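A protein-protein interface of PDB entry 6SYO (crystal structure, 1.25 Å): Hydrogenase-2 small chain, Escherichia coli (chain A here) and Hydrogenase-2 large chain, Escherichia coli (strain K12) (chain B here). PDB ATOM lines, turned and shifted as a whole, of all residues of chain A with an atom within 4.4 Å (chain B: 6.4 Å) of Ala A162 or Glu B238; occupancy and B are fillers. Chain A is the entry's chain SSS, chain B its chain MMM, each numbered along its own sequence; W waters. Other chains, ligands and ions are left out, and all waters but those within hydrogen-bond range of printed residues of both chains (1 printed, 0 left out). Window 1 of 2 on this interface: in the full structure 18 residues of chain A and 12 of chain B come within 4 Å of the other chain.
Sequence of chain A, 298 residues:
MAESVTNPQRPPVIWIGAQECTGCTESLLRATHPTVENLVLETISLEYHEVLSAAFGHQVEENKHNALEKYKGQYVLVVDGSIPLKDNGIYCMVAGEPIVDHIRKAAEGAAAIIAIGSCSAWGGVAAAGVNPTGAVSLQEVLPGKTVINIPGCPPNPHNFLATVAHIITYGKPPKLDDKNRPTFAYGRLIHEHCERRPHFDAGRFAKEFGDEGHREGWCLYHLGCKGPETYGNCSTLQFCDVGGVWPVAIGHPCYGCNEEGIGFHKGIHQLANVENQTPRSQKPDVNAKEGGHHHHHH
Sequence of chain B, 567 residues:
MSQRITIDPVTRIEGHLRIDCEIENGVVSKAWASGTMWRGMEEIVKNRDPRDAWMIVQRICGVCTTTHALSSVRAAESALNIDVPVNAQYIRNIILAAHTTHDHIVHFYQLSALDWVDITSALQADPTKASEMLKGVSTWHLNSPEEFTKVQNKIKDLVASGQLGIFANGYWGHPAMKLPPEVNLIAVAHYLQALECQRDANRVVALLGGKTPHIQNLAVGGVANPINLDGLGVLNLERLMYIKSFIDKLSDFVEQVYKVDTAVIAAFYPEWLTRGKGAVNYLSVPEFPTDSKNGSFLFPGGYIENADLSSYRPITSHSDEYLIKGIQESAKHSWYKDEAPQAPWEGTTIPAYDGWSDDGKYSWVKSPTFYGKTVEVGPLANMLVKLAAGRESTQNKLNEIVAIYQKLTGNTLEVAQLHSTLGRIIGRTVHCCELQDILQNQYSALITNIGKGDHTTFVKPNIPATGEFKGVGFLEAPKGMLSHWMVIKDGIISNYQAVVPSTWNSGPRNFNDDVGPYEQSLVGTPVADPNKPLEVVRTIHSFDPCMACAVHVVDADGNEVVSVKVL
Of chain B, only Leu B237 (3.9 Å), Glu B238 (3.9 Å) and Met B241 (3.9 Å) come within 4 Å of Ala A162. Of the printed residues of chain B, Phe A184 touches Leu B229 (3.8 Å). Of the printed residues of chain B, Leu A237 touches Glu B238 and Arg B239. Val B234 touches none of the printed residues of chain A. Of chain A, only His A33, His A158, Ala A162 and Leu A237 come within 4 Å of Glu B238. Of the printed residues of chain A, Arg B239 touches Leu A237. Of the printed residues of chain A, Met B241 touches His A33 (3.5 Å), Ala A162 (3.9 Å) and Ala A165 (3.6 Å). Of the printed residues of chain A, Tyr B242 touches His A33. The nearest printed residue of chain A that does not touch Glu B238 is Phe A184 (4.4 Å). The nearest printed residue of chain B that does not touch His A158 is Met B241 (6.2 Å).
Water W1 lies within hydrogen-bond range of O of His A33 (2.9 Å) and SD of Met B241 (3.4 Å).
A ring nitrogen (NE2) of His A33 lies within hydrogen-bond range of the side-chain carboxylate of Glu B238 (2.6 Å).
CE of Met B241 touches O of His A33, at 3.5 Å. His A33 touches Tyr B242 (ND1 to CD1, 3.3 Å). Glu B238 touches His A158. Leu B237 touches Ala A162. Glu B238 touches Ala A162. Ala A162 touches Met B241. Leu B237 touches Ala A165 (CD2 to C, 3.99 Å). Met B241 touches Ala A165 (SD to CB, 3.6 Å). CB of Phe A184 touches O of Leu B229, 3.8 Å away. CD1 of Leu A237 touches OE2 of Glu B238, 3.4 Å away.
Printed residues of chain B that touch a printed residue of chain A: Leu B229, Leu B237, Glu B238, Arg B239, Met B241 and Tyr B242. Printed residues of chain A that touch a printed residue of chain B: His A33, His A158, Ala A162, Ala A165, His A166, Phe A184 and Leu A237. Among the printed residues, no Asp or Glu carboxylate lies within 4 Å of a Lys or Arg side-chain nitrogen of the other chain.
A ring nitrogen (ND1) of His A33 sits at hydrogen-bond distance from a ring nitrogen (NE2) of His A158, 3.2 Å away. The side-chain amide oxygen (OD1) of Asn B236 sits at hydrogen-bond distance from the backbone NH (N) of Glu B238 (3.2 Å). N of Arg B239 is in hydrogen-bond range of OD1 of Asn B236, at 3.0 Å. The guanidinium group of Arg B239 lies within salt-bridge range of the side-chain carboxylate of Glu B238 (2.9 Å).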
ATOM      1  N   HIS A  33      11.459  15.107   4.927  1.00  0.00           N
ATOM      2  CA  HIS A  33      12.693  14.966   5.764  1.00  0.00           C
ATOM      3  C   HIS A  33      13.936  15.293   4.933  1.00  0.00           C
ATOM      4  O   HIS A  33      14.739  14.385   4.580  1.00  0.00           O
ATOM      5  CB  HIS A  33      12.745  13.569   6.455  1.00  0.00           C
ATOM      6  CG  HIS A  33      12.551  12.358   5.593  1.00  0.00           C
ATOM      7  ND1 HIS A  33      11.279  11.994   5.105  1.00  0.00           N
ATOM      8  CD2 HIS A  33      13.412  11.356   5.183  1.00  0.00           C
ATOM      9  CE1 HIS A  33      11.421  10.824   4.457  1.00  0.00           C
ATOM     10  NE2 HIS A  33      12.699  10.397   4.497  1.00  0.00           N
ATOM     11  N   HIS A 158      13.513  12.188  -1.748  1.00  0.00           N
ATOM     12  CA  HIS A 158      14.565  11.858  -0.769  1.00  0.00           C
ATOM     13  C   HIS A 158      15.724  11.083  -1.434  1.00  0.00           C
ATOM     14  O   HIS A 158      16.845  11.021  -0.866  1.00  0.00           O
ATOM     15  CB  HIS A 158      14.009  11.120   0.474  1.00  0.00           C
ATOM     16  CG  HIS A 158      12.869  11.862   1.114  1.00  0.00           C
ATOM     17  ND1 HIS A 158      11.556  11.588   0.806  1.00  0.00           N
ATOM     18  CD2 HIS A 158      12.836  12.946   1.949  1.00  0.00           C
ATOM     19  CE1 HIS A 158      10.786  12.491   1.494  1.00  0.00           C
ATOM     20  NE2 HIS A 158      11.511  13.335   2.202  1.00  0.00           N
ATOM     21  N   PHE A 160      17.196  12.280  -3.991  1.00  0.00           N
ATOM     22  CA  PHE A 160      17.970  13.544  -4.149  1.00  0.00           C
ATOM     23  C   PHE A 160      18.407  14.108  -2.790  1.00  0.00           C
ATOM     24  O   PHE A 160      19.643  14.380  -2.577  1.00  0.00           O
ATOM     25  CB  PHE A 160      17.173  14.560  -4.977  1.00  0.00           C
ATOM     26  CG  PHE A 160      17.719  15.981  -4.950  1.00  0.00           C
ATOM     27  CD1 PHE A 160      18.837  16.314  -5.736  1.00  0.00           C
ATOM     28  CD2 PHE A 160      17.161  16.967  -4.159  1.00  0.00           C
ATOM     29  CE1 PHE A 160      19.349  17.607  -5.713  1.00  0.00           C
ATOM     30  CE2 PHE A 160      17.687  18.275  -4.113  1.00  0.00           C
ATOM     31  CZ  PHE A 160      18.784  18.589  -4.914  1.00  0.00           C
ATOM     32  N   LEU A 161      17.496  14.285  -1.844  1.00  0.00           N
ATOM     33  CA  LEU A 161      17.802  14.999  -0.590  1.00  0.00           C
ATOM     34  C   LEU A 161      18.850  14.247   0.250  1.00  0.00           C
ATOM     35  O   LEU A 161      19.749  14.873   0.852  1.00  0.00           O
ATOM     36  CB  LEU A 161      16.512  15.250   0.243  1.00  0.00           C
ATOM     37  CG  LEU A 161      15.523  16.229  -0.424  1.00  0.00           C
ATOM     38  CD1 LEU A 161      14.118  16.091   0.174  1.00  0.00           C
ATOM     39  CD2 LEU A 161      16.005  17.659  -0.346  1.00  0.00           C
ATOM     40  N   ALA A 162      18.778  12.899   0.297  1.00  0.00           N
ATOM     41  CA  ALA A 162      19.760  12.081   1.080  1.00  0.00           C
ATOM     42  C   ALA A 162      21.116  12.059   0.354  1.00  0.00           C
ATOM     43  O   ALA A 162      22.162  11.842   1.056  1.00  0.00           O
ATOM     44  CB  ALA A 162      19.233  10.704   1.391  1.00  0.00           C
ATOM     45  N   THR A 163      21.165  12.246  -0.959  1.00  0.00           N
ATOM     46  CA  THR A 163      22.453  12.381  -1.700  1.00  0.00           C
ATOM     47  C   THR A 163      23.104  13.722  -1.308  1.00  0.00           C
ATOM     48  O   THR A 163      24.344  13.707  -0.951  1.00  0.00           O
ATOM     49  CB  THR A 163      22.220  12.248  -3.202  1.00  0.00           C
ATOM     50  OG1 THR A 163      21.781  10.890  -3.516  1.00  0.00           O
ATOM     51  CG2 THR A 163      23.480  12.522  -4.035  1.00  0.00           C
ATOM     52  N   VAL A 164      22.349  14.827  -1.346  1.00  0.00           N
ATOM     53  CA  VAL A 164      22.862  16.131  -0.907  1.00  0.00           C
ATOM     54  C   VAL A 164      23.325  16.044   0.565  1.00  0.00           C
ATOM     55  O   VAL A 164      24.417  16.575   0.918  1.00  0.00           O
ATOM     56  CB  VAL A 164      21.834  17.218  -1.208  1.00  0.00           C
ATOM     57  CG1 VAL A 164      22.237  18.560  -0.583  1.00  0.00           C
ATOM     58  CG2 VAL A 164      21.584  17.395  -2.686  1.00  0.00           C
ATOM     59  N   ALA A 165      22.539  15.462   1.437  1.00  0.00           N
ATOM     60  CA  ALA A 165      22.886  15.341   2.868  1.00  0.00           C
ATOM     61  C   ALA A 165      24.204  14.555   3.048  1.00  0.00           C
ATOM     62  O   ALA A 165      24.978  14.905   3.955  1.00  0.00           O
ATOM     63  CB  ALA A 165      21.764  14.666   3.677  1.00  0.00           C
ATOM     64  N   HIS A 166      24.436  13.513   2.250  1.00  0.00           N
ATOM     65  CA  HIS A 166      25.690  12.746   2.414  1.00  0.00           C
ATOM     66  C   HIS A 166      26.857  13.674   2.084  1.00  0.00           C
ATOM     67  O   HIS A 166      27.919  13.638   2.830  1.00  0.00           O
ATOM     68  CB  HIS A 166      25.650  11.472   1.520  1.00  0.00           C
ATOM     69  CG  HIS A 166      26.717  10.477   1.835  1.00  0.00           C
ATOM     70  ND1 HIS A 166      28.081  10.645   1.557  1.00  0.00           N
ATOM     71  CD2 HIS A 166      26.629   9.279   2.472  1.00  0.00           C
ATOM     72  CE1 HIS A 166      28.719   9.539   1.914  1.00  0.00           C
ATOM     73  NE2 HIS A 166      27.903   8.676   2.507  1.00  0.00           N
ATOM     74  N   PHE A 184      22.107   3.261  -2.528  1.00  0.00           N
ATOM     75  CA  PHE A 184      21.039   3.137  -1.480  1.00  0.00           C
ATOM     76  C   PHE A 184      19.663   3.173  -2.152  1.00  0.00           C
ATOM     77  O   PHE A 184      18.688   2.671  -1.540  1.00  0.00           O
ATOM     78  CB  PHE A 184      21.108   4.177  -0.338  1.00  0.00           C
ATOM     79  CG  PHE A 184      20.621   5.559  -0.713  1.00  0.00           C
ATOM     80  CD1 PHE A 184      21.464   6.528  -1.283  1.00  0.00           C
ATOM     81  CD2 PHE A 184      19.274   5.917  -0.477  1.00  0.00           C
ATOM     82  CE1 PHE A 184      20.957   7.776  -1.643  1.00  0.00           C
ATOM     83  CE2 PHE A 184      18.801   7.192  -0.830  1.00  0.00           C
ATOM     84  CZ  PHE A 184      19.632   8.119  -1.403  1.00  0.00           C
ATOM     85  N   LEU A 237      11.176   2.094  -0.449  1.00  0.00           N
ATOM     86  CA  LEU A 237      10.939   3.507  -0.059  1.00  0.00           C
ATOM     87  C   LEU A 237       9.547   3.934  -0.502  1.00  0.00           C
ATOM     88  O   LEU A 237       8.900   4.736   0.234  1.00  0.00           O
ATOM     89  CB  LEU A 237      12.066   4.388  -0.609  1.00  0.00           C
ATOM     90  CG  LEU A 237      11.935   5.851  -0.137  1.00  0.00           C
ATOM     91  CD1 LEU A 237      12.025   5.919   1.430  1.00  0.00           C
ATOM     92  CD2 LEU A 237      13.046   6.731  -0.761  1.00  0.00           C
ATOM     93  N   LEU B 229      24.886   3.073   5.371  1.00  0.00           N
ATOM     94  CA  LEU B 229      24.430   4.331   4.729  1.00  0.00           C
ATOM     95  C   LEU B 229      24.156   4.189   3.271  1.00  0.00           C
ATOM     96  O   LEU B 229      23.322   4.973   2.701  1.00  0.00           O
ATOM     97  CB  LEU B 229      25.423   5.483   4.929  1.00  0.00           C
ATOM     98  CG  LEU B 229      25.648   5.900   6.387  1.00  0.00           C
ATOM     99  CD1 LEU B 229      26.400   7.205   6.437  1.00  0.00           C
ATOM    100  CD2 LEU B 229      24.372   6.059   7.230  1.00  0.00           C
ATOM    101  N   VAL B 234      17.696  -1.068   4.307  1.00  0.00           N
ATOM    102  CA  VAL B 234      18.307  -1.154   5.647  1.00  0.00           C
ATOM    103  C   VAL B 234      18.393   0.239   6.294  1.00  0.00           C
ATOM    104  O   VAL B 234      17.765   1.209   5.755  1.00  0.00           O
ATOM    105  CB  VAL B 234      19.659  -1.888   5.537  1.00  0.00           C
ATOM    106  CG1 VAL B 234      19.516  -3.321   4.949  1.00  0.00           C
ATOM    107  CG2 VAL B 234      20.697  -1.093   4.758  1.00  0.00           C
ATOM    108  N   ASN B 236      19.768   3.356   6.558  1.00  0.00           N
ATOM    109  CA  ASN B 236      20.634   4.197   5.717  1.00  0.00           C
ATOM    110  C   ASN B 236      20.458   5.672   6.097  1.00  0.00           C
ATOM    111  O   ASN B 236      19.782   6.001   7.091  1.00  0.00           O
ATOM    112  CB  ASN B 236      20.414   3.860   4.241  1.00  0.00           C
ATOM    113  CG  ASN B 236      18.992   4.157   3.799  1.00  0.00           C
ATOM    114  OD1 ASN B 236      18.335   5.060   4.360  1.00  0.00           O
ATOM    115  ND2 ASN B 236      18.499   3.493   2.730  1.00  0.00           N
ATOM    116  N   LEU B 237      21.108   6.581   5.358  1.00  0.00           N
ATOM    117  CA  LEU B 237      21.043   8.008   5.761  1.00  0.00           C
ATOM    118  C   LEU B 237      19.614   8.575   5.583  1.00  0.00           C
ATOM    119  O   LEU B 237      19.160   9.397   6.416  1.00  0.00           O
ATOM    120  CB  LEU B 237      22.060   8.847   5.009  1.00  0.00           C
ATOM    121  CG  LEU B 237      22.229  10.304   5.505  1.00  0.00           C
ATOM    122  CD1 LEU B 237      22.616  10.376   7.008  1.00  0.00           C
ATOM    123  CD2 LEU B 237      23.313  11.015   4.658  1.00  0.00           C
ATOM    124  N   GLU B 238      18.882   8.170   4.547  1.00  0.00           N
ATOM    125  CA  GLU B 238      17.480   8.628   4.361  1.00  0.00           C
ATOM    126  C   GLU B 238      16.603   8.237   5.593  1.00  0.00           C
ATOM    127  O   GLU B 238      15.800   9.053   6.092  1.00  0.00           O
ATOM    128  CB  GLU B 238      16.920   8.046   3.037  1.00  0.00           C
ATOM    129  CG  GLU B 238      15.451   8.409   2.776  1.00  0.00           C
ATOM    130  CD  GLU B 238      14.483   7.472   3.481  1.00  0.00           C
ATOM    131  OE1 GLU B 238      14.758   6.244   3.606  1.00  0.00           O
ATOM    132  OE2 GLU B 238      13.330   7.929   3.833  1.00  0.00           O
ATOM    133  N   ARG B 239      16.748   6.983   6.071  1.00  0.00           N
ATOM    134  CA  ARG B 239      15.949   6.522   7.239  1.00  0.00           C
ATOM    135  C   ARG B 239      16.353   7.324   8.500  1.00  0.00           C
ATOM    136  O   ARG B 239      15.452   7.739   9.305  1.00  0.00           O
ATOM    137  CB  ARG B 239      16.142   5.023   7.472  1.00  0.00           C
ATOM    138  CG  ARG B 239      15.621   4.058   6.387  1.00  0.00           C
ATOM    139  CD  ARG B 239      14.090   3.800   6.379  1.00  0.00           C
ATOM    140  NE  ARG B 239      13.372   4.875   5.721  1.00  0.00           N
ATOM    141  CZ  ARG B 239      12.025   4.963   5.712  1.00  0.00           C
ATOM    142  NH1 ARG B 239      11.283   4.073   6.372  1.00  0.00           N
ATOM    143  NH2 ARG B 239      11.449   5.955   5.013  1.00  0.00           N
ATOM    144  N   LEU B 240      17.665   7.575   8.677  1.00  0.00           N
ATOM    145  CA  LEU B 240      18.124   8.378   9.841  1.00  0.00           C
ATOM    146  C   LEU B 240      17.580   9.816   9.772  1.00  0.00           C
ATOM    147  O   LEU B 240      17.102  10.348  10.811  1.00  0.00           O
ATOM    148  CB  LEU B 240      19.673   8.339   9.890  1.00  0.00           C
ATOM    149  CG  LEU B 240      20.227   6.995  10.348  1.00  0.00           C
ATOM    150  CD1 LEU B 240      21.714   6.868  10.012  1.00  0.00           C
ATOM    151  CD2 LEU B 240      20.037   6.763  11.849  1.00  0.00           C
ATOM    152  N   MET B 241      17.569  10.437   8.571  1.00  0.00           N
ATOM    153  CA  MET B 241      16.962  11.783   8.416  1.00  0.00           C
ATOM    154  C   MET B 241      15.486  11.770   8.811  1.00  0.00           C
ATOM    155  O   MET B 241      14.973  12.744   9.373  1.00  0.00           O
ATOM    156  CB  MET B 241      17.146  12.267   6.978  1.00  0.00           C
ATOM    157  CG  MET B 241      18.638  12.535   6.591  1.00  0.00           C
ATOM    158  SD  MET B 241      18.948  12.793   4.846  1.00  0.00           S
ATOM    159  CE  MET B 241      18.252  14.448   4.574  1.00  0.00           C
ATOM    160  N   TYR B 242      14.786  10.690   8.441  1.00  0.00           N
ATOM    161  CA  TYR B 242      13.333  10.587   8.786  1.00  0.00           C
ATOM    162  C   TYR B 242      13.155  10.547  10.317  1.00  0.00           C
ATOM    163  O   TYR B 242      12.288  11.263  10.886  1.00  0.00           O
ATOM    164  CB  TYR B 242      12.713   9.361   8.084  1.00  0.00           C
ATOM    165  CG  TYR B 242      11.206   9.336   7.929  1.00  0.00           C
ATOM    166  CD1 TYR B 242      10.418  10.480   7.877  1.00  0.00           C
ATOM    167  CD2 TYR B 242      10.565   8.116   7.680  1.00  0.00           C
ATOM    168  CE1 TYR B 242       9.048  10.419   7.606  1.00  0.00           C
ATOM    169  CE2 TYR B 242       9.186   8.032   7.452  1.00  0.00           C
ATOM    170  CZ  TYR B 242       8.441   9.191   7.367  1.00  0.00           C
ATOM    171  OH  TYR B 242       7.069   9.145   7.116  1.00  0.00           O
ATOM    172  N   ILE B 243      13.949   9.723  11.024  1.00  0.00           N
ATOM    173  CA  ILE B 243      13.945   9.685  12.506  1.00  0.00           C
ATOM    174  C   ILE B 243      14.150  11.113  13.037  1.00  0.00           C
ATOM    175  O   ILE B 243      13.410  11.559  13.974  1.00  0.00           O
ATOM    176  CB  ILE B 243      15.016   8.693  13.005  1.00  0.00           C
ATOM    177  CG1 ILE B 243      14.593   7.256  12.649  1.00  0.00           C
ATOM    178  CG2 ILE B 243      15.262   8.860  14.497  1.00  0.00           C
ATOM    179  CD1 ILE B 243      15.739   6.234  12.640  1.00  0.00           C
HETATM  180  O   HOH W   1      16.105  12.212   3.148  1.00  0.00           O
